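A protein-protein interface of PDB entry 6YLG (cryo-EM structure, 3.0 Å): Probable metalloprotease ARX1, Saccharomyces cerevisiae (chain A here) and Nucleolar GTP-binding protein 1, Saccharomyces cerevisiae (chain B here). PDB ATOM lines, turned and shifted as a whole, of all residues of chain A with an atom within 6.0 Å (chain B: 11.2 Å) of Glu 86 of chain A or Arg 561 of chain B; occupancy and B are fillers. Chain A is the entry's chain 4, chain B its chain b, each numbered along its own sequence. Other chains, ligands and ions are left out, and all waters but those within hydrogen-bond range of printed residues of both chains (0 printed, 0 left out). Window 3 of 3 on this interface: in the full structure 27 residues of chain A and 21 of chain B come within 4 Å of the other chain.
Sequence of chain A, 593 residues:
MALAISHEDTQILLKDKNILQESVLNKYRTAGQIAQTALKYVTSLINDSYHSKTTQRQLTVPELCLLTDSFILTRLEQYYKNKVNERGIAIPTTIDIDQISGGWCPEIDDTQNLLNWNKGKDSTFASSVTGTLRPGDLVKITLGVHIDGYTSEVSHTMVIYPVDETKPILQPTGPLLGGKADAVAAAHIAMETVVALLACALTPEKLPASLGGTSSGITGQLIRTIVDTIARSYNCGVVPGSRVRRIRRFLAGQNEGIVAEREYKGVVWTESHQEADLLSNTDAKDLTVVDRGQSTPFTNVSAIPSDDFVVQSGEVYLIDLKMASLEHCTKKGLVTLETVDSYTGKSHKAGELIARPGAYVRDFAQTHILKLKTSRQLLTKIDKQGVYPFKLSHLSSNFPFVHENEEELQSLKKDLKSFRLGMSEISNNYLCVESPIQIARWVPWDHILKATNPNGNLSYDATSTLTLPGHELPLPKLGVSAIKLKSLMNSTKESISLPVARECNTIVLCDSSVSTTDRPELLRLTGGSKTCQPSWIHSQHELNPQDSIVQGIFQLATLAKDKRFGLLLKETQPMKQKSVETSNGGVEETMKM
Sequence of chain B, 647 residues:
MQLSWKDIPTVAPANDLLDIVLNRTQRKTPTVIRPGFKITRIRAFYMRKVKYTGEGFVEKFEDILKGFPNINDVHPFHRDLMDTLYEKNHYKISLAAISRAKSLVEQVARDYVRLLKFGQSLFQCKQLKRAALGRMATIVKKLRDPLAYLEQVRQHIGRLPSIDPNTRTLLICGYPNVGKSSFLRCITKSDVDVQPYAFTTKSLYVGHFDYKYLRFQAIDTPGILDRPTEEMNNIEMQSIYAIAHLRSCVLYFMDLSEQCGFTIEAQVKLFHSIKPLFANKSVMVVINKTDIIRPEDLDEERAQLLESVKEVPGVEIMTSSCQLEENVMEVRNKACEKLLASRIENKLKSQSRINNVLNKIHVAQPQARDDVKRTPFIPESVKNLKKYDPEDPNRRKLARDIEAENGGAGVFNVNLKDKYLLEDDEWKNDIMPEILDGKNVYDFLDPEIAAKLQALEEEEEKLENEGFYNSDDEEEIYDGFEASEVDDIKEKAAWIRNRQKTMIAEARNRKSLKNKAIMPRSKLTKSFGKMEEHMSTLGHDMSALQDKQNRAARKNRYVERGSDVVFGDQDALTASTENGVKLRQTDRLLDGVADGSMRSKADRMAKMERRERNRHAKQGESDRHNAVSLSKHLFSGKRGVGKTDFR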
ATOM      1  N   ASN A  85     -33.565 -14.647 -23.480  1.00  0.00           N
ATOM      2  CA  ASN A  85     -33.900 -14.558 -22.064  1.00  0.00           C
ATOM      3  C   ASN A  85     -32.691 -14.896 -21.198  1.00  0.00           C
ATOM      4  O   ASN A  85     -32.492 -14.303 -20.138  1.00  0.00           O
ATOM      5  CB  ASN A  85     -35.067 -15.488 -21.732  1.00  0.00           C
ATOM      6  CG  ASN A  85     -36.340 -15.101 -22.454  1.00  0.00           C
ATOM      7  OD1 ASN A  85     -36.308 -14.693 -23.615  1.00  0.00           O
ATOM      8  ND2 ASN A  85     -37.470 -15.218 -21.768  1.00  0.00           N
ATOM      9  N   GLU A  86     -31.889 -15.856 -21.652  1.00  0.00           N
ATOM     10  CA  GLU A  86     -30.635 -16.199 -20.992  1.00  0.00           C
ATOM     11  C   GLU A  86     -29.606 -15.132 -21.342  1.00  0.00           C
ATOM     12  O   GLU A  86     -29.182 -15.024 -22.497  1.00  0.00           O
ATOM     13  CB  GLU A  86     -30.159 -17.586 -21.416  1.00  0.00           C
ATOM     14  CG  GLU A  86     -30.876 -18.726 -20.714  1.00  0.00           C
ATOM     15  CD  GLU A  86     -30.194 -19.142 -19.426  1.00  0.00           C
ATOM     16  OE1 GLU A  86     -28.998 -19.497 -19.470  1.00  0.00           O
ATOM     17  OE2 GLU A  86     -30.856 -19.117 -18.367  1.00  0.00           O
ATOM     18  N   ARG A  87     -29.207 -14.346 -20.348  1.00  0.00           N
ATOM     19  CA  ARG A  87     -28.298 -13.232 -20.569  1.00  0.00           C
ATOM     20  C   ARG A  87     -27.639 -12.874 -19.247  1.00  0.00           C
ATOM     21  O   ARG A  87     -28.290 -12.906 -18.200  1.00  0.00           O
ATOM     22  CB  ARG A  87     -29.043 -12.018 -21.136  1.00  0.00           C
ATOM     23  CG  ARG A  87     -30.002 -11.375 -20.148  1.00  0.00           C
ATOM     24  CD  ARG A  87     -31.219 -10.796 -20.842  1.00  0.00           C
ATOM     25  NE  ARG A  87     -32.023  -9.984 -19.931  1.00  0.00           N
ATOM     26  CZ  ARG A  87     -31.745  -8.730 -19.580  1.00  0.00           C
ATOM     27  NH1 ARG A  87     -30.674  -8.103 -20.051  1.00  0.00           N
ATOM     28  NH2 ARG A  87     -32.550  -8.090 -18.743  1.00  0.00           N
ATOM     29  N   GLY A  88     -26.354 -12.540 -19.301  1.00  0.00           N
ATOM     30  CA  GLY A  88     -25.649 -12.132 -18.106  1.00  0.00           C
ATOM     31  C   GLY A  88     -24.142 -12.142 -18.240  1.00  0.00           C
ATOM     32  O   GLY A  88     -23.603 -11.906 -19.325  1.00  0.00           O
ATOM     33  N   HIS A 146     -22.403 -12.297 -21.947  1.00  0.00           N
ATOM     34  CA  HIS A 146     -23.064 -13.223 -22.854  1.00  0.00           C
ATOM     35  C   HIS A 146     -24.546 -12.901 -22.955  1.00  0.00           C
ATOM     36  O   HIS A 146     -25.169 -12.434 -21.998  1.00  0.00           O
ATOM     37  CB  HIS A 146     -22.873 -14.676 -22.402  1.00  0.00           C
ATOM     38  CG  HIS A 146     -23.910 -15.150 -21.432  1.00  0.00           C
ATOM     39  ND1 HIS A 146     -25.055 -15.805 -21.829  1.00  0.00           N
ATOM     40  CD2 HIS A 146     -23.972 -15.066 -20.083  1.00  0.00           C
ATOM     41  CE1 HIS A 146     -25.780 -16.102 -20.765  1.00  0.00           C
ATOM     42  NE2 HIS A 146     -25.145 -15.665 -19.694  1.00  0.00           N
ATOM     43  N   ILE A 147     -25.092 -13.148 -24.144  1.00  0.00           N
ATOM     44  CA  ILE A 147     -26.505 -12.957 -24.446  1.00  0.00           C
ATOM     45  C   ILE A 147     -26.968 -14.160 -25.255  1.00  0.00           C
ATOM     46  O   ILE A 147     -26.448 -14.415 -26.346  1.00  0.00           O
ATOM     47  CB  ILE A 147     -26.765 -11.654 -25.230  1.00  0.00           C
ATOM     48  CG1 ILE A 147     -26.371 -10.421 -24.407  1.00  0.00           C
ATOM     49  CG2 ILE A 147     -28.230 -11.578 -25.639  1.00  0.00           C
ATOM     50  CD1 ILE A 147     -26.240  -9.147 -25.217  1.00  0.00           C
ATOM     51  N   ASP A 148     -27.946 -14.892 -24.723  1.00  0.00           N
ATOM     52  CA  ASP A 148     -28.501 -16.102 -25.322  1.00  0.00           C
ATOM     53  C   ASP A 148     -27.434 -17.122 -25.698  1.00  0.00           C
ATOM     54  O   ASP A 148     -27.590 -17.833 -26.699  1.00  0.00           O
ATOM     55  CB  ASP A 148     -29.346 -15.774 -26.558  1.00  0.00           C
ATOM     56  CG  ASP A 148     -30.431 -16.801 -26.812  1.00  0.00           C
ATOM     57  OD1 ASP A 148     -31.420 -16.827 -26.052  1.00  0.00           O
ATOM     58  OD2 ASP A 148     -30.293 -17.586 -27.774  1.00  0.00           O
ATOM     59  N   GLY A 149     -26.353 -17.220 -24.922  1.00  0.00           N
ATOM     60  CA  GLY A 149     -25.264 -18.130 -25.183  1.00  0.00           C
ATOM     61  C   GLY A 149     -24.166 -17.549 -26.051  1.00  0.00           C
ATOM     62  O   GLY A 149     -23.061 -18.101 -26.087  1.00  0.00           O
ATOM     63  N   PHE A 250     -23.305 -20.967 -26.251  1.00  0.00           N
ATOM     64  CA  PHE A 250     -23.136 -21.518 -24.906  1.00  0.00           C
ATOM     65  C   PHE A 250     -21.815 -22.258 -24.711  1.00  0.00           C
ATOM     66  O   PHE A 250     -21.546 -22.729 -23.599  1.00  0.00           O
ATOM     67  CB  PHE A 250     -24.288 -22.461 -24.513  1.00  0.00           C
ATOM     68  CG  PHE A 250     -25.576 -21.758 -24.158  1.00  0.00           C
ATOM     69  CD1 PHE A 250     -25.629 -20.828 -23.133  1.00  0.00           C
ATOM     70  CD2 PHE A 250     -26.741 -22.052 -24.841  1.00  0.00           C
ATOM     71  CE1 PHE A 250     -26.813 -20.196 -22.812  1.00  0.00           C
ATOM     72  CE2 PHE A 250     -27.926 -21.423 -24.520  1.00  0.00           C
ATOM     73  CZ  PHE A 250     -27.960 -20.495 -23.505  1.00  0.00           C
ATOM     74  N   ASP A 383     -29.430 -22.390 -10.500  1.00  0.00           N
ATOM     75  CA  ASP A 383     -29.864 -22.977 -11.763  1.00  0.00           C
ATOM     76  C   ASP A 383     -30.831 -22.081 -12.527  1.00  0.00           C
ATOM     77  O   ASP A 383     -31.063 -22.336 -13.713  1.00  0.00           O
ATOM     78  CB  ASP A 383     -30.498 -24.366 -11.566  1.00  0.00           C
ATOM     79  CG  ASP A 383     -31.438 -24.442 -10.381  1.00  0.00           C
ATOM     80  OD1 ASP A 383     -31.742 -25.553  -9.923  1.00  0.00           O
ATOM     81  OD2 ASP A 383     -31.880 -23.374  -9.906  1.00  0.00           O
ATOM     82  N   LYS A 384     -31.377 -21.030 -11.903  1.00  0.00           N
ATOM     83  CA  LYS A 384     -32.077 -20.021 -12.689  1.00  0.00           C
ATOM     84  C   LYS A 384     -31.091 -19.123 -13.429  1.00  0.00           C
ATOM     85  O   LYS A 384     -31.441 -18.515 -14.447  1.00  0.00           O
ATOM     86  CB  LYS A 384     -33.013 -19.208 -11.796  1.00  0.00           C
ATOM     87  CG  LYS A 384     -34.281 -19.969 -11.413  1.00  0.00           C
ATOM     88  CD  LYS A 384     -35.458 -19.041 -11.175  1.00  0.00           C
ATOM     89  CE  LYS A 384     -36.714 -19.813 -10.777  1.00  0.00           C
ATOM     90  NZ  LYS A 384     -37.093 -20.883 -11.749  1.00  0.00           N
ATOM     91  N   GLN A 385     -29.857 -19.026 -12.935  1.00  0.00           N
ATOM     92  CA  GLN A 385     -28.765 -18.537 -13.764  1.00  0.00           C
ATOM     93  C   GLN A 385     -28.301 -19.652 -14.697  1.00  0.00           C
ATOM     94  O   GLN A 385     -28.869 -20.747 -14.722  1.00  0.00           O
ATOM     95  CB  GLN A 385     -27.598 -18.031 -12.912  1.00  0.00           C
ATOM     96  CG  GLN A 385     -27.995 -17.000 -11.867  1.00  0.00           C
ATOM     97  CD  GLN A 385     -26.961 -15.898 -11.682  1.00  0.00           C
ATOM     98  OE1 GLN A 385     -25.788 -16.060 -12.022  1.00  0.00           O
ATOM     99  NE2 GLN A 385     -27.398 -14.768 -11.138  1.00  0.00           N
ATOM    100  N   GLY A 386     -27.247 -19.368 -15.459  1.00  0.00           N
ATOM    101  CA  GLY A 386     -26.838 -20.255 -16.532  1.00  0.00           C
ATOM    102  C   GLY A 386     -25.657 -21.143 -16.210  1.00  0.00           C
ATOM    103  O   GLY A 386     -25.314 -21.353 -15.043  1.00  0.00           O
ATOM    104  N   VAL A 387     -25.025 -21.671 -17.262  1.00  0.00           N
ATOM    105  CA  VAL A 387     -23.896 -22.583 -17.120  1.00  0.00           C
ATOM    106  C   VAL A 387     -22.572 -21.864 -16.914  1.00  0.00           C
ATOM    107  O   VAL A 387     -21.535 -22.535 -16.781  1.00  0.00           O
ATOM    108  CB  VAL A 387     -23.784 -23.512 -18.347  1.00  0.00           C
ATOM    109  CG1 VAL A 387     -25.119 -24.160 -18.634  1.00  0.00           C
ATOM    110  CG2 VAL A 387     -23.290 -22.737 -19.565  1.00  0.00           C
ATOM    111  N   ARG B 557     -44.504 -28.377 -24.655  1.00  0.00           N
ATOM    112  CA  ARG B 557     -43.157 -28.505 -25.201  1.00  0.00           C
ATOM    113  C   ARG B 557     -42.226 -27.430 -24.638  1.00  0.00           C
ATOM    114  O   ARG B 557     -42.659 -26.428 -24.061  1.00  0.00           O
ATOM    115  CB  ARG B 557     -43.189 -28.479 -26.737  1.00  0.00           C
ATOM    116  CG  ARG B 557     -43.351 -27.123 -27.437  1.00  0.00           C
ATOM    117  CD  ARG B 557     -44.724 -26.511 -27.232  1.00  0.00           C
ATOM    118  NE  ARG B 557     -45.138 -25.711 -28.383  1.00  0.00           N
ATOM    119  CZ  ARG B 557     -44.585 -24.558 -28.753  1.00  0.00           C
ATOM    120  NH1 ARG B 557     -43.573 -24.029 -28.073  1.00  0.00           N
ATOM    121  NH2 ARG B 557     -45.051 -23.926 -29.821  1.00  0.00           N
ATOM    122  N   TYR B 558     -40.922 -27.653 -24.826  1.00  0.00           N
ATOM    123  CA  TYR B 558     -39.881 -27.010 -24.032  1.00  0.00           C
ATOM    124  C   TYR B 558     -39.040 -26.072 -24.892  1.00  0.00           C
ATOM    125  O   TYR B 558     -39.189 -26.012 -26.116  1.00  0.00           O
ATOM    126  CB  TYR B 558     -38.976 -28.059 -23.362  1.00  0.00           C
ATOM    127  CG  TYR B 558     -38.349 -29.048 -24.323  1.00  0.00           C
ATOM    128  CD1 TYR B 558     -37.101 -28.810 -24.882  1.00  0.00           C
ATOM    129  CD2 TYR B 558     -39.003 -30.223 -24.666  1.00  0.00           C
ATOM    130  CE1 TYR B 558     -36.525 -29.710 -25.757  1.00  0.00           C
ATOM    131  CE2 TYR B 558     -38.436 -31.129 -25.540  1.00  0.00           C
ATOM    132  CZ  TYR B 558     -37.196 -30.867 -26.083  1.00  0.00           C
ATOM    133  OH  TYR B 558     -36.623 -31.766 -26.953  1.00  0.00           O
ATOM    134  N   VAL B 559     -38.142 -25.346 -24.216  1.00  0.00           N
ATOM    135  CA  VAL B 559     -37.329 -24.315 -24.859  1.00  0.00           C
ATOM    136  C   VAL B 559     -35.859 -24.727 -24.974  1.00  0.00           C
ATOM    137  O   VAL B 559     -35.067 -24.012 -25.599  1.00  0.00           O
ATOM    138  CB  VAL B 559     -37.471 -22.986 -24.093  1.00  0.00           C
ATOM    139  CG1 VAL B 559     -38.935 -22.697 -23.796  1.00  0.00           C
ATOM    140  CG2 VAL B 559     -36.657 -23.010 -22.804  1.00  0.00           C
ATOM    141  N   GLU B 560     -35.464 -25.860 -24.383  1.00  0.00           N
ATOM    142  CA  GLU B 560     -34.106 -26.380 -24.517  1.00  0.00           C
ATOM    143  C   GLU B 560     -33.053 -25.414 -23.981  1.00  0.00           C
ATOM    144  O   GLU B 560     -32.293 -24.820 -24.752  1.00  0.00           O
ATOM    145  CB  GLU B 560     -33.809 -26.729 -25.981  1.00  0.00           C
ATOM    146  CG  GLU B 560     -32.497 -27.490 -26.215  1.00  0.00           C
ATOM    147  CD  GLU B 560     -32.446 -28.834 -25.509  1.00  0.00           C
ATOM    148  OE1 GLU B 560     -31.330 -29.351 -25.290  1.00  0.00           O
ATOM    149  OE2 GLU B 560     -33.520 -29.374 -25.173  1.00  0.00           O
ATOM    150  N   ARG B 561     -33.028 -25.231 -22.662  1.00  0.00           N
ATOM    151  CA  ARG B 561     -32.068 -24.357 -22.002  1.00  0.00           C
ATOM    152  C   ARG B 561     -30.628 -24.774 -22.311  1.00  0.00           C
ATOM    153  O   ARG B 561     -30.359 -25.838 -22.874  1.00  0.00           O
ATOM    154  CB  ARG B 561     -32.285 -24.371 -20.489  1.00  0.00           C
ATOM    155  CG  ARG B 561     -33.690 -23.971 -20.035  1.00  0.00           C
ATOM    156  CD  ARG B 561     -33.840 -24.035 -18.515  1.00  0.00           C
ATOM    157  NE  ARG B 561     -32.782 -23.305 -17.821  1.00  0.00           N
ATOM    158  CZ  ARG B 561     -32.680 -21.979 -17.773  1.00  0.00           C
ATOM    159  NH1 ARG B 561     -33.573 -21.199 -18.372  1.00  0.00           N
ATOM    160  NH2 ARG B 561     -31.672 -21.424 -17.116  1.00  0.00           N
ATOM    161  N   GLY B 562     -29.689 -23.906 -21.928  1.00  0.00           N
ATOM    162  CA  GLY B 562     -28.288 -24.172 -22.211  1.00  0.00           C
ATOM    163  C   GLY B 562     -27.689 -25.209 -21.281  1.00  0.00           C
ATOM    164  O   GLY B 562     -26.714 -25.881 -21.627  1.00  0.00           O
ATOM    165  N   SER B 563     -28.240 -25.327 -20.070  1.00  0.00           N
ATOM    166  CA  SER B 563     -27.878 -26.435 -19.190  1.00  0.00           C
ATOM    167  C   SER B 563     -27.991 -27.769 -19.909  1.00  0.00           C
ATOM    168  O   SER B 563     -27.094 -28.616 -19.802  1.00  0.00           O
ATOM    169  CB  SER B 563     -28.782 -26.436 -17.957  1.00  0.00           C
ATOM    170  OG  SER B 563     -29.100 -25.119 -17.546  1.00  0.00           O
ATOM    171  N   ASP B 564     -29.071 -27.958 -20.667  1.00  0.00           N
ATOM    172  CA  ASP B 564     -29.226 -29.178 -21.447  1.00  0.00           C
ATOM    173  C   ASP B 564     -28.118 -29.312 -22.483  1.00  0.00           C
ATOM    174  O   ASP B 564     -27.413 -30.324 -22.507  1.00  0.00           O
ATOM    175  CB  ASP B 564     -30.590 -29.199 -22.134  1.00  0.00           C
ATOM    176  CG  ASP B 564     -31.734 -28.989 -21.162  1.00  0.00           C
ATOM    177  OD1 ASP B 564     -32.154 -27.826 -20.980  1.00  0.00           O
ATOM    178  OD2 ASP B 564     -32.218 -29.985 -20.585  1.00  0.00           O
ATOM    179  N   VAL B 565     -27.915 -28.280 -23.310  1.00  0.00           N
ATOM    180  CA  VAL B 565     -27.010 -28.402 -24.450  1.00  0.00           C
ATOM    181  C   VAL B 565     -25.582 -28.647 -23.978  1.00  0.00           C
ATOM    182  O   VAL B 565     -24.775 -29.253 -24.694  1.00  0.00           O
ATOM    183  CB  VAL B 565     -27.117 -27.152 -25.349  1.00  0.00           C
ATOM    184  CG1 VAL B 565     -26.228 -26.007 -24.867  1.00  0.00           C
ATOM    185  CG2 VAL B 565     -26.785 -27.513 -26.793  1.00  0.00           C
ATOM    186  N   VAL B 566     -25.247 -28.188 -22.769  1.00  0.00           N
ATOM    187  CA  VAL B 566     -23.928 -28.485 -22.219  1.00  0.00           C
ATOM    188  C   VAL B 566     -23.889 -29.885 -21.613  1.00  0.00           C
ATOM    189  O   VAL B 566     -23.079 -30.720 -22.026  1.00  0.00           O
ATOM    190  CB  VAL B 566     -23.513 -27.416 -21.185  1.00  0.00           C
ATOM    191  CG1 VAL B 566     -22.118 -27.719 -20.631  1.00  0.00           C
ATOM    192  CG2 VAL B 566     -23.554 -26.024 -21.811  1.00  0.00           C
ATOM    193  N   PHE B 567     -24.761 -30.172 -20.637  1.00  0.00           N
ATOM    194  CA  PHE B 567     -24.561 -31.311 -19.746  1.00  0.00           C
ATOM    195  C   PHE B 567     -25.578 -32.432 -19.945  1.00  0.00           C
ATOM    196  O   PHE B 567     -25.810 -33.224 -19.028  1.00  0.00           O
ATOM    197  CB  PHE B 567     -24.607 -30.829 -18.294  1.00  0.00           C
ATOM    198  CG  PHE B 567     -23.465 -29.935 -17.905  1.00  0.00           C
ATOM    199  CD1 PHE B 567     -22.160 -30.398 -17.915  1.00  0.00           C
ATOM    200  CD2 PHE B 567     -23.699 -28.628 -17.526  1.00  0.00           C
ATOM    201  CE1 PHE B 567     -21.120 -29.568 -17.555  1.00  0.00           C
ATOM    202  CE2 PHE B 567     -22.664 -27.800 -17.164  1.00  0.00           C
ATOM    203  CZ  PHE B 567     -21.373 -28.270 -17.180  1.00  0.00           C
ATOM    204  N   GLY B 568     -26.188 -32.528 -21.124  1.00  0.00           N
ATOM    205  CA  GLY B 568     -27.072 -33.647 -21.381  1.00  0.00           C
ATOM    206  C   GLY B 568     -26.273 -34.890 -21.698  1.00  0.00           C
ATOM    207  O   GLY B 568     -26.331 -35.896 -20.984  1.00  0.00           O
ATOM    208  N   ASP B 569     -25.517 -34.811 -22.792  1.00  0.00           N
ATOM    209  CA  ASP B 569     -24.594 -35.881 -23.155  1.00  0.00           C
ATOM    210  C   ASP B 569     -23.557 -36.140 -22.068  1.00  0.00           C
ATOM    211  O   ASP B 569     -23.254 -37.301 -21.769  1.00  0.00           O
ATOM    212  CB  ASP B 569     -23.895 -35.533 -24.471  1.00  0.00           C
ATOM    213  CG  ASP B 569     -23.292 -34.137 -24.464  1.00  0.00           C
ATOM    214  OD1 ASP B 569     -23.323 -33.476 -23.404  1.00  0.00           O
ATOM    215  OD2 ASP B 569     -22.805 -33.696 -25.523  1.00  0.00           O
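Arg 561 of chain B touches just these residues of chain A: Glu 86 (2.7 Å), Asp 383 (3.6 Å), Lys 384 (3.95 Å) and Gln 385 (3.7 Å). Asn 85 of chain A touches none of the printed residues of chain B. No residue of chain B comes within 4 Å of Gly 88 of chain A. Ile 147 of chain A touches none of the printed residues of chain B. No residue of chain B comes within 4 Å of Gly 386 of chain A. Of the printed residues of chain B, Val 387 of chain A touches Gly 562 (3.8 Å), Ser 563 (3.6 Å) and Val 566 (3.99 Å). Of the printed residues of chain B, Phe 250 of chain A touches Gly 562 and Val 565. Of the printed residues of chain A, Val 566 of chain B touches Val 387 (3.99 Å). Tyr 558 of chain B touches none of the printed residues of chain A.
Phe 250 of chain A touches Gly 562 of chain B. Phe 250 of chain A touches Val 565 of chain B. Arg 561 of chain B touches Asp 383 of chain A. NH2 of Arg 561 of chain B touches O of Lys 384 of chain A (3.95 Å). Arg 561 of chain B touches Gln 385 of chain A. Val 387 of chain A touches Gly 562 of chain B (CG1 to O, 3.8 Å). CA of Ser 563 of chain B touches CG1 of Val 387 of chain A, at 3.6 Å. Val 387 of chain A touches Val 566 of chain B (CG2 to CG2, 3.99 Å).
Of the 14 printed residues of chain A, 6 touch a printed residue of chain B. Hydrophobic or aromatic side chains of chain A within 4 Å of the printed part of chain B: Phe 250 and Val 387. Hydrophobic or aromatic side chains of chain B within 4 Å of the printed part of chain A: Val 565 and Val 566.
N of Arg 561 of chain B lies within hydrogen-bond range of OD1 of Asp 564 of chain B (3.2 Å). The backbone carbonyl oxygen (O) of Glu 86 of chain A lies within hydrogen-bond range of the backbone NH (N) of Asp 148 of chain A, at 2.5 Å. The backbone carbonyl oxygen (O) of Gly 149 of chain A lies within hydrogen-bond range of the backbone NH (N) of Phe 250 of chain A, 2.9 Å away.
The guanidinium group (NH2) of Arg 561 of chain B is in salt-bridge range of the side-chain carboxylate (OE2) of Glu 86 of chain A (2.7 Å).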
